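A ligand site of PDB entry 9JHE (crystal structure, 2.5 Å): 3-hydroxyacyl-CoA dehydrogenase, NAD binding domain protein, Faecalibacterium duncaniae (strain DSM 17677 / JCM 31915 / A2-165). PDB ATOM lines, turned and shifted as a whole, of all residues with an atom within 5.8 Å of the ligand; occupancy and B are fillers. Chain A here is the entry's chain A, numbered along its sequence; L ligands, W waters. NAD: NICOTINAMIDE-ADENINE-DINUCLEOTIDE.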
ATOM      1  N   ILE A   6      23.835  15.093  21.976  1.00  0.00           N
ATOM      2  CA  ILE A   6      24.411  15.466  23.267  1.00  0.00           C
ATOM      3  C   ILE A   6      24.513  14.213  24.120  1.00  0.00           C
ATOM      4  O   ILE A   6      23.500  13.637  24.524  1.00  0.00           O
ATOM      5  CB  ILE A   6      23.569  16.541  23.955  1.00  0.00           C
ATOM      6  CG1 ILE A   6      23.050  17.549  22.934  1.00  0.00           C
ATOM      7  CG2 ILE A   6      24.394  17.249  25.019  1.00  0.00           C
ATOM      8  CD1 ILE A   6      24.133  18.394  22.299  1.00  0.00           C
ATOM      9  N   GLY A   7      25.736  13.779  24.413  1.00  0.00           N
ATOM     10  CA  GLY A   7      25.942  12.527  25.112  1.00  0.00           C
ATOM     11  C   GLY A   7      26.484  11.447  24.189  1.00  0.00           C
ATOM     12  O   GLY A   7      25.841  11.092  23.201  1.00  0.00           O
ATOM     13  N   ALA A   8      27.671  10.929  24.498  1.00  0.00           N
ATOM     14  CA  ALA A   8      28.371   9.955  23.665  1.00  0.00           C
ATOM     15  C   ALA A   8      28.419   8.585  24.337  1.00  0.00           C
ATOM     16  O   ALA A   8      29.399   7.858  24.238  1.00  0.00           O
ATOM     17  CB  ALA A   8      29.779  10.433  23.340  1.00  0.00           C
ATOM     18  N   GLY A   9      27.340   8.221  25.012  1.00  0.00           N
ATOM     19  CA  GLY A   9      27.221   6.955  25.693  1.00  0.00           C
ATOM     20  C   GLY A   9      26.568   5.901  24.829  1.00  0.00           C
ATOM     21  O   GLY A   9      26.690   5.894  23.607  1.00  0.00           O
ATOM     22  N   THR A  10      25.841   4.990  25.491  1.00  0.00           N
ATOM     23  CA  THR A  10      25.221   3.866  24.791  1.00  0.00           C
ATOM     24  C   THR A  10      24.230   4.349  23.749  1.00  0.00           C
ATOM     25  O   THR A  10      24.230   3.882  22.607  1.00  0.00           O
ATOM     26  CB  THR A  10      24.542   2.940  25.793  1.00  0.00           C
ATOM     27  OG1 THR A  10      25.455   2.625  26.856  1.00  0.00           O
ATOM     28  CG2 THR A  10      24.104   1.655  25.113  1.00  0.00           C
ATOM     29  N   MET A  11      23.364   5.297  24.113  1.00  0.00           N
ATOM     30  CA  MET A  11      22.341   5.763  23.197  1.00  0.00           C
ATOM     31  C   MET A  11      22.864   6.849  22.260  1.00  0.00           C
ATOM     32  O   MET A  11      22.441   6.920  21.104  1.00  0.00           O
ATOM     33  CB  MET A  11      21.123   6.270  23.958  1.00  0.00           C
ATOM     34  CG  MET A  11      20.526   5.245  24.910  1.00  0.00           C
ATOM     35  SD  MET A  11      19.844   3.818  24.047  1.00  0.00           S
ATOM     36  CE  MET A  11      18.899   4.618  22.752  1.00  0.00           C
ATOM     37  N   GLY A  12      23.748   7.712  22.745  1.00  0.00           N
ATOM     38  CA  GLY A  12      24.356   8.691  21.866  1.00  0.00           C
ATOM     39  C   GLY A  12      25.089   8.057  20.703  1.00  0.00           C
ATOM     40  O   GLY A  12      25.018   8.535  19.577  1.00  0.00           O
ATOM     41  N   CYS A  30      28.809  15.004  21.004  1.00  0.00           N
ATOM     42  CA  CYS A  30      29.333  15.780  22.117  1.00  0.00           C
ATOM     43  C   CYS A  30      29.202  14.997  23.417  1.00  0.00           C
ATOM     44  O   CYS A  30      28.430  14.043  23.534  1.00  0.00           O
ATOM     45  CB  CYS A  30      28.602  17.123  22.232  1.00  0.00           C
ATOM     46  SG  CYS A  30      28.304  17.924  20.641  1.00  0.00           S
ATOM     47  N   ASP A  31      29.980  15.428  24.416  1.00  0.00           N
ATOM     48  CA  ASP A  31      29.999  14.777  25.720  1.00  0.00           C
ATOM     49  C   ASP A  31      30.590  15.745  26.739  1.00  0.00           C
ATOM     50  O   ASP A  31      30.841  16.913  26.429  1.00  0.00           O
ATOM     51  CB  ASP A  31      30.779  13.456  25.660  1.00  0.00           C
ATOM     52  CG  ASP A  31      30.259  12.432  26.651  1.00  0.00           C
ATOM     53  OD1 ASP A  31      30.328  12.699  27.862  1.00  0.00           O
ATOM     54  OD2 ASP A  31      29.791  11.362  26.214  1.00  0.00           O
ATOM     55  N   ILE A  32      30.823  15.255  27.969  1.00  0.00           N
ATOM     56  CA  ILE A  32      31.306  16.119  29.038  1.00  0.00           C
ATOM     57  C   ILE A  32      32.676  16.683  28.703  1.00  0.00           C
ATOM     58  O   ILE A  32      32.916  17.892  28.774  1.00  0.00           O
ATOM     59  CB  ILE A  32      31.299  15.371  30.380  1.00  0.00           C
ATOM     60  CG1 ILE A  32      31.880  13.956  30.229  1.00  0.00           C
ATOM     61  CG2 ILE A  32      29.894  15.306  30.951  1.00  0.00           C
ATOM     62  CD1 ILE A  32      32.697  13.476  31.422  1.00  0.00           C
ATOM     63  N   TRP A  36      36.267  12.025  26.419  1.00  0.00           N
ATOM     64  CA  TRP A  36      35.097  11.191  26.622  1.00  0.00           C
ATOM     65  C   TRP A  36      34.227  11.114  25.378  1.00  0.00           C
ATOM     66  O   TRP A  36      33.445  10.171  25.233  1.00  0.00           O
ATOM     67  CB  TRP A  36      34.269  11.691  27.801  1.00  0.00           C
ATOM     68  CG  TRP A  36      34.761  11.206  29.140  1.00  0.00           C
ATOM     69  CD1 TRP A  36      35.696  11.809  29.936  1.00  0.00           C
ATOM     70  CD2 TRP A  36      34.339  10.025  29.828  1.00  0.00           C
ATOM     71  NE1 TRP A  36      35.871  11.071  31.079  1.00  0.00           N
ATOM     72  CE2 TRP A  36      35.054   9.971  31.045  1.00  0.00           C
ATOM     73  CE3 TRP A  36      33.429   9.002  29.544  1.00  0.00           C
ATOM     74  CZ2 TRP A  36      34.893   8.939  31.966  1.00  0.00           C
ATOM     75  CZ3 TRP A  36      33.264   7.984  30.467  1.00  0.00           C
ATOM     76  CH2 TRP A  36      33.991   7.956  31.660  1.00  0.00           C
ATOM     77  N   LYS A  74      29.988  20.286  22.847  1.00  0.00           N
ATOM     78  CA  LYS A  74      29.093  21.301  22.236  1.00  0.00           C
ATOM     79  C   LYS A  74      29.685  22.698  22.431  1.00  0.00           C
ATOM     80  O   LYS A  74      30.801  22.788  22.969  1.00  0.00           O
ATOM     81  CB  LYS A  74      27.699  21.228  22.842  1.00  0.00           C
ATOM     82  CG  LYS A  74      27.556  21.711  24.279  1.00  0.00           C
ATOM     83  CD  LYS A  74      27.031  20.660  25.221  1.00  0.00           C
ATOM     84  CE  LYS A  74      28.102  20.015  26.060  1.00  0.00           C
ATOM     85  NZ  LYS A  74      28.686  18.823  25.395  1.00  0.00           N
ATOM     86  N   GLU A  86      19.369  15.117  22.589  1.00  0.00           N
ATOM     87  CA  GLU A  86      20.172  14.874  23.785  1.00  0.00           C
ATOM     88  C   GLU A  86      20.075  13.408  24.200  1.00  0.00           C
ATOM     89  O   GLU A  86      19.039  12.760  24.041  1.00  0.00           O
ATOM     90  CB  GLU A  86      19.717  15.784  24.927  1.00  0.00           C
ATOM     91  CG  GLU A  86      18.394  15.396  25.581  1.00  0.00           C
ATOM     92  CD  GLU A  86      18.572  14.480  26.771  1.00  0.00           C
ATOM     93  OE1 GLU A  86      19.595  14.607  27.474  1.00  0.00           O
ATOM     94  OE2 GLU A  86      17.687  13.627  27.013  1.00  0.00           O
ATOM     95  N   ALA A  87      21.190  12.886  24.719  1.00  0.00           N
ATOM     96  CA  ALA A  87      21.283  11.530  25.258  1.00  0.00           C
ATOM     97  C   ALA A  87      22.038  11.558  26.580  1.00  0.00           C
ATOM     98  O   ALA A  87      22.916  10.727  26.836  1.00  0.00           O
ATOM     99  CB  ALA A  87      21.957  10.583  24.269  1.00  0.00           C
ATOM    100  N   ALA A  88      21.731  12.535  27.422  1.00  0.00           N
ATOM    101  CA  ALA A  88      22.497  12.793  28.636  1.00  0.00           C
ATOM    102  C   ALA A  88      21.922  11.997  29.808  1.00  0.00           C
ATOM    103  O   ALA A  88      21.065  11.138  29.649  1.00  0.00           O
ATOM    104  CB  ALA A  88      22.531  14.293  28.917  1.00  0.00           C
ATOM    105  N   PHE A  89      22.418  12.291  31.012  1.00  0.00           N
ATOM    106  CA  PHE A  89      21.999  11.569  32.202  1.00  0.00           C
ATOM    107  C   PHE A  89      20.522  11.800  32.493  1.00  0.00           C
ATOM    108  O   PHE A  89      19.973  12.875  32.219  1.00  0.00           O
ATOM    109  CB  PHE A  89      22.841  11.993  33.408  1.00  0.00           C
ATOM    110  CG  PHE A  89      24.289  11.615  33.320  1.00  0.00           C
ATOM    111  CD1 PHE A  89      25.269  12.546  33.615  1.00  0.00           C
ATOM    112  CD2 PHE A  89      24.663  10.335  32.939  1.00  0.00           C
ATOM    113  CE1 PHE A  89      26.612  12.199  33.535  1.00  0.00           C
ATOM    114  CE2 PHE A  89      25.998   9.994  32.858  1.00  0.00           C
ATOM    115  CZ  PHE A  89      26.975  10.923  33.162  1.00  0.00           C
ATOM    116  N   GLU A  90      19.873  10.777  33.045  1.00  0.00           N
ATOM    117  CA  GLU A  90      18.454  10.858  33.386  1.00  0.00           C
ATOM    118  C   GLU A  90      18.331  11.672  34.660  1.00  0.00           C
ATOM    119  O   GLU A  90      18.150  11.161  35.771  1.00  0.00           O
ATOM    120  CB  GLU A  90      17.848   9.461  33.522  1.00  0.00           C
ATOM    121  CG  GLU A  90      16.328   9.462  33.626  1.00  0.00           C
ATOM    122  CD  GLU A  90      15.633   9.546  32.271  1.00  0.00           C
ATOM    123  OE1 GLU A  90      16.077  10.323  31.403  1.00  0.00           O
ATOM    124  OE2 GLU A  90      14.620   8.827  32.076  1.00  0.00           O
ATOM    125  N   VAL A  94      20.052  18.359  34.719  1.00  0.00           N
ATOM    126  CA  VAL A  94      21.107  18.112  33.745  1.00  0.00           C
ATOM    127  C   VAL A  94      20.608  18.431  32.342  1.00  0.00           C
ATOM    128  O   VAL A  94      21.234  19.172  31.581  1.00  0.00           O
ATOM    129  CB  VAL A  94      21.627  16.670  33.847  1.00  0.00           C
ATOM    130  CG1 VAL A  94      22.264  16.235  32.530  1.00  0.00           C
ATOM    131  CG2 VAL A  94      22.624  16.546  34.986  1.00  0.00           C
ATOM    132  N   LYS A  95      19.446  17.863  31.976  1.00  0.00           N
ATOM    133  CA  LYS A  95      18.864  18.176  30.681  1.00  0.00           C
ATOM    134  C   LYS A  95      18.351  19.609  30.623  1.00  0.00           C
ATOM    135  O   LYS A  95      18.326  20.212  29.547  1.00  0.00           O
ATOM    136  CB  LYS A  95      17.729  17.193  30.373  1.00  0.00           C
ATOM    137  CG  LYS A  95      18.105  15.728  30.589  1.00  0.00           C
ATOM    138  CD  LYS A  95      17.076  14.797  29.962  1.00  0.00           C
ATOM    139  CE  LYS A  95      17.315  13.349  30.368  1.00  0.00           C
ATOM    140  NZ  LYS A  95      18.475  12.742  29.665  1.00  0.00           N
ATOM    141  N   THR A  98      21.474  21.647  30.114  1.00  0.00           N
ATOM    142  CA  THR A  98      21.964  21.456  28.761  1.00  0.00           C
ATOM    143  C   THR A  98      21.085  22.192  27.751  1.00  0.00           C
ATOM    144  O   THR A  98      21.593  23.001  26.956  1.00  0.00           O
ATOM    145  CB  THR A  98      22.026  19.961  28.452  1.00  0.00           C
ATOM    146  OG1 THR A  98      22.782  19.288  29.480  1.00  0.00           O
ATOM    147  CG2 THR A  98      22.681  19.693  27.117  1.00  0.00           C
ATOM    148  N   ASN A 115      15.772  12.408  24.298  1.00  0.00           N
ATOM    149  CA  ASN A 115      15.645  10.964  24.229  1.00  0.00           C
ATOM    150  C   ASN A 115      15.146  10.352  25.538  1.00  0.00           C
ATOM    151  O   ASN A 115      15.069   9.120  25.633  1.00  0.00           O
ATOM    152  CB  ASN A 115      16.996  10.344  23.846  1.00  0.00           C
ATOM    153  CG  ASN A 115      16.880   8.901  23.413  1.00  0.00           C
ATOM    154  OD1 ASN A 115      15.929   8.520  22.725  1.00  0.00           O
ATOM    155  ND2 ASN A 115      17.831   8.076  23.828  1.00  0.00           N
ATOM    156  N   THR A 116      14.798  11.161  26.530  1.00  0.00           N
ATOM    157  CA  THR A 116      14.451  10.651  27.850  1.00  0.00           C
ATOM    158  C   THR A 116      13.259   9.680  27.782  1.00  0.00           C
ATOM    159  O   THR A 116      12.457   9.698  26.851  1.00  0.00           O
ATOM    160  CB  THR A 116      14.131  11.799  28.803  1.00  0.00           C
ATOM    161  OG1 THR A 116      14.215  11.336  30.153  1.00  0.00           O
ATOM    162  CG2 THR A 116      12.732  12.348  28.538  1.00  0.00           C
ATOM    163  N   SER A 117      13.178   8.822  28.796  1.00  0.00           N
ATOM    164  CA  SER A 117      12.110   7.846  28.904  1.00  0.00           C
ATOM    165  C   SER A 117      11.230   8.029  30.129  1.00  0.00           C
ATOM    166  O   SER A 117      10.070   7.596  30.101  1.00  0.00           O
ATOM    167  CB  SER A 117      12.692   6.417  28.946  1.00  0.00           C
ATOM    168  OG  SER A 117      13.810   6.308  28.085  1.00  0.00           O
ATOM    169  N   SER A 118      11.731   8.658  31.186  1.00  0.00           N
ATOM    170  CA  SER A 118      10.995   8.809  32.438  1.00  0.00           C
ATOM    171  C   SER A 118      10.832  10.256  32.863  1.00  0.00           C
ATOM    172  O   SER A 118      10.178  10.511  33.883  1.00  0.00           O
ATOM    173  CB  SER A 118      11.694   8.013  33.554  1.00  0.00           C
ATOM    174  OG  SER A 118      13.055   8.394  33.671  1.00  0.00           O
ATOM    175  N   HIS A 136      12.088   9.441  21.302  1.00  0.00           N
ATOM    176  CA  HIS A 136      12.457   8.272  22.109  1.00  0.00           C
ATOM    177  C   HIS A 136      12.983   7.173  21.199  1.00  0.00           C
ATOM    178  O   HIS A 136      12.216   6.485  20.529  1.00  0.00           O
ATOM    179  CB  HIS A 136      11.265   7.795  22.928  1.00  0.00           C
ATOM    180  CG  HIS A 136      11.632   6.846  24.021  1.00  0.00           C
ATOM    181  ND1 HIS A 136      10.922   5.685  24.267  1.00  0.00           N
ATOM    182  CD2 HIS A 136      12.628   6.870  24.935  1.00  0.00           C
ATOM    183  CE1 HIS A 136      11.470   5.049  25.287  1.00  0.00           C
ATOM    184  NE2 HIS A 136      12.505   5.743  25.703  1.00  0.00           N
ATOM    185  N   PHE A 137      14.306   7.006  21.187  1.00  0.00           N
ATOM    186  CA  PHE A 137      14.923   5.891  20.493  1.00  0.00           C
ATOM    187  C   PHE A 137      14.902   4.648  21.377  1.00  0.00           C
ATOM    188  O   PHE A 137      14.642   4.718  22.580  1.00  0.00           O
ATOM    189  CB  PHE A 137      16.369   6.231  20.094  1.00  0.00           C
ATOM    190  CG  PHE A 137      16.470   7.116  18.887  1.00  0.00           C
ATOM    191  CD1 PHE A 137      16.248   8.477  18.992  1.00  0.00           C
ATOM    192  CD2 PHE A 137      16.805   6.578  17.654  1.00  0.00           C
ATOM    193  CE1 PHE A 137      16.348   9.289  17.881  1.00  0.00           C
ATOM    194  CE2 PHE A 137      16.906   7.390  16.542  1.00  0.00           C
ATOM    195  CZ  PHE A 137      16.679   8.743  16.645  1.00  0.00           C
ATOM    196  N   PHE A 138      15.193   3.503  20.771  1.00  0.00           N
ATOM    197  CA  PHE A 138      15.197   2.223  21.463  1.00  0.00           C
ATOM    198  C   PHE A 138      16.514   1.521  21.183  1.00  0.00           C
ATOM    199  O   PHE A 138      16.887   1.345  20.026  1.00  0.00           O
ATOM    200  CB  PHE A 138      14.006   1.352  21.044  1.00  0.00           C
ATOM    201  CG  PHE A 138      12.684   1.861  21.550  1.00  0.00           C
ATOM    202  CD1 PHE A 138      12.040   2.917  20.933  1.00  0.00           C
ATOM    203  CD2 PHE A 138      12.080   1.268  22.648  1.00  0.00           C
ATOM    204  CE1 PHE A 138      10.824   3.382  21.395  1.00  0.00           C
ATOM    205  CE2 PHE A 138      10.868   1.726  23.122  1.00  0.00           C
ATOM    206  CZ  PHE A 138      10.240   2.787  22.502  1.00  0.00           C
ATOM    207  N   ASN A 139      17.201   1.107  22.240  1.00  0.00           N
ATOM    208  CA  ASN A 139      18.521   0.518  22.099  1.00  0.00           C
ATOM    209  C   ASN A 139      18.427  -0.875  21.478  1.00  0.00           C
ATOM    210  O   ASN A 139      17.594  -1.686  21.910  1.00  0.00           O
ATOM    211  CB  ASN A 139      19.212   0.432  23.464  1.00  0.00           C
ATOM    212  CG  ASN A 139      20.597  -0.166  23.379  1.00  0.00           C
ATOM    213  OD1 ASN A 139      21.480   0.374  22.724  1.00  0.00           O
ATOM    214  ND2 ASN A 139      20.782  -1.297  24.046  1.00  0.00           N
HETATM  215  PA  NAD L   1      25.068   6.587  29.296  1.00  0.00           P
HETATM  216  O1A NAD L   1      25.584   6.835  30.684  1.00  0.00           O
HETATM  217  O2A NAD L   1      25.919   5.544  28.607  1.00  0.00           O
HETATM  218  O5B NAD L   1      25.124   8.028  28.416  1.00  0.00           O
HETATM  219  C5B NAD L   1      25.290   9.234  29.131  1.00  0.00           C
HETATM  220  C4B NAD L   1      26.369  10.071  28.396  1.00  0.00           C
HETATM  221  O4B NAD L   1      25.989  11.328  28.315  1.00  0.00           O
HETATM  222  C3B NAD L   1      27.697  10.061  29.225  1.00  0.00           C
HETATM  223  O3B NAD L   1      28.729   9.743  28.436  1.00  0.00           O
HETATM  224  C2B NAD L   1      27.846  11.518  29.759  1.00  0.00           C
HETATM  225  O2B NAD L   1      29.296  11.885  29.876  1.00  0.00           O
HETATM  226  C1B NAD L   1      27.255  12.239  28.834  1.00  0.00           C
HETATM  227  N9A NAD L   1      26.788  13.499  29.372  1.00  0.00           N
HETATM  228  C8A NAD L   1      26.324  13.713  30.597  1.00  0.00           C
HETATM  229  N7A NAD L   1      26.002  14.980  30.746  1.00  0.00           N
HETATM  230  C5A NAD L   1      26.263  15.609  29.588  1.00  0.00           C
HETATM  231  C6A NAD L   1      26.138  16.914  29.136  1.00  0.00           C
HETATM  232  N6A NAD L   1      25.608  17.956  30.013  1.00  0.00           N
HETATM  233  N1A NAD L   1      26.490  17.212  27.913  1.00  0.00           N
HETATM  234  C2A NAD L   1      26.965  16.267  27.118  1.00  0.00           C
HETATM  235  N3A NAD L   1      27.108  15.031  27.492  1.00  0.00           N
HETATM  236  C4A NAD L   1      26.769  14.662  28.719  1.00  0.00           C
HETATM  237  O3  NAD L   1      23.501   6.060  29.357  1.00  0.00           O
HETATM  238  PN  NAD L   1      22.457   6.142  28.053  1.00  0.00           P
HETATM  239  O1N NAD L   1      21.771   4.815  27.878  1.00  0.00           O
HETATM  240  O2N NAD L   1      23.242   6.479  26.784  1.00  0.00           O
HETATM  241  O5D NAD L   1      21.306   7.346  28.331  1.00  0.00           O
HETATM  242  C5D NAD L   1      20.962   8.242  27.248  1.00  0.00           C
HETATM  243  C4D NAD L   1      19.486   8.778  27.472  1.00  0.00           C
HETATM  244  O4D NAD L   1      18.662   8.068  26.820  1.00  0.00           O
HETATM  245  C3D NAD L   1      19.075   8.639  28.993  1.00  0.00           C
HETATM  246  O3D NAD L   1      18.444   9.794  29.418  1.00  0.00           O
HETATM  247  C2D NAD L   1      18.126   7.501  29.033  1.00  0.00           C
HETATM  248  O2D NAD L   1      17.123   7.692  30.136  1.00  0.00           O
HETATM  249  C1D NAD L   1      17.533   7.568  27.854  1.00  0.00           C
HETATM  250  N1N NAD L   1      17.012   6.255  27.463  1.00  0.00           N
HETATM  251  C2N NAD L   1      18.070   5.185  27.508  1.00  0.00           C
HETATM  252  C3N NAD L   1      17.446   3.826  27.200  1.00  0.00           C
HETATM  253  C7N NAD L   1      18.556   2.752  27.178  1.00  0.00           C
HETATM  254  O7N NAD L   1      19.591   2.977  27.708  1.00  0.00           O
HETATM  255  N7N NAD L   1      18.307   1.456  26.503  1.00  0.00           N
HETATM  256  C4N NAD L   1      16.739   3.804  25.854  1.00  0.00           C
HETATM  257  C5N NAD L   1      15.808   4.971  25.624  1.00  0.00           C
HETATM  258  C6N NAD L   1      16.358   6.328  26.110  1.00  0.00           C
HETATM  259  O   HOH W   1      28.147   4.503  28.268  1.00  0.00           O
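O of Ala 87 lies close to O4B of the ligand, at 3.5 Å.
The side-chain hydroxyl of Ser 117 lies close to a nitrogen (N1N) of the ligand.
Merely in contact with the ligand: Phe 137 (3.3 Å), Phe 89 (3.3 Å), Ile 32 (3.3 Å), Asn 139 (3.3 Å), His 136 (3.4 Å), Gly 7 (3.4 Å), Ile 6 (3.5 Å), Gly 9 (3.5 Å) and Lys 74 (3.5 Å).
Hydrophobic or aromatic side chains that line the ligand: Ile 6, Met 11, Ile 32, Ala 87, Ala 88, Phe 89 and His 136.
Of the 28 residues printed, 19 come within 4 Å of the ligand.
OD1 of Asp 31 is in hydrogen-bond range of O2B of the ligand, 2.4 Å away.
N of Met 11 is in hydrogen-bond range of O2N of the ligand, at 2.9 Å.
The side-chain sulfur of Met 11 lies close to a nitrogen (N7N) of the ligand.
The backbone carbonyl oxygen (O) of Ala 88 sits at hydrogen-bond distance from an oxygen (O3D) of the ligand (3.0 Å).
O3D of the ligand sits at hydrogen-bond distance from NZ of Lys 95 (3.0 Å).
The side-chain carboxylate (OE1) of Glu 90 is in hydrogen-bond range of an oxygen (O2D) of the ligand, 3.1 Å away.
An oxygen (O4D) of the ligand sits at hydrogen-bond distance from the side-chain amide nitrogen (ND2) of Asn 115 (3.1 Å).
An oxygen (O2A) of the ligand sits at hydrogen-bond distance from the backbone NH (N) of Thr 10.
The side-chain hydroxyl of Thr 10 sits at hydrogen-bond distance from an oxygen (O2A) of the ligand (3.4 Å).
The side-chain hydroxyl (OG1) of Thr 98 lies within hydrogen-bond range of a nitrogen (N6A) of the ligand (3.2 Å).
The side-chain amino group (NZ) of Lys 74 sits at hydrogen-bond distance from the backbone carbonyl oxygen (O) of Asp 31, at 3.1 Å.
The side-chain amino group of Lys 95 lies within salt-bridge range of the side-chain carboxylate of Glu 90, 3.8 Å away.
The side-chain amino group (NZ) of Lys 95 is in salt-bridge range of the side-chain carboxylate (OE2) of Glu 86 (2.9 Å).
The side-chain carboxylate (OE1) of Glu 90 is in hydrogen-bond range of the side-chain hydroxyl (OG1) of Thr 116.
The backbone carbonyl oxygen (O) of Glu 86 lies close to the backbone NH (N) of Asn 115.
The side-chain hydroxyl (OG1) of Thr 98 sits at hydrogen-bond distance from the backbone carbonyl oxygen (O) of Val 94 (2.6 Å).
N of Ala 87 is in hydrogen-bond range of O of Ile 6 (2.4 Å).
The backbone NH (N) of Lys 74 sits close to the side-chain sulfur (SG) of Cys 30 (3.6 Å).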
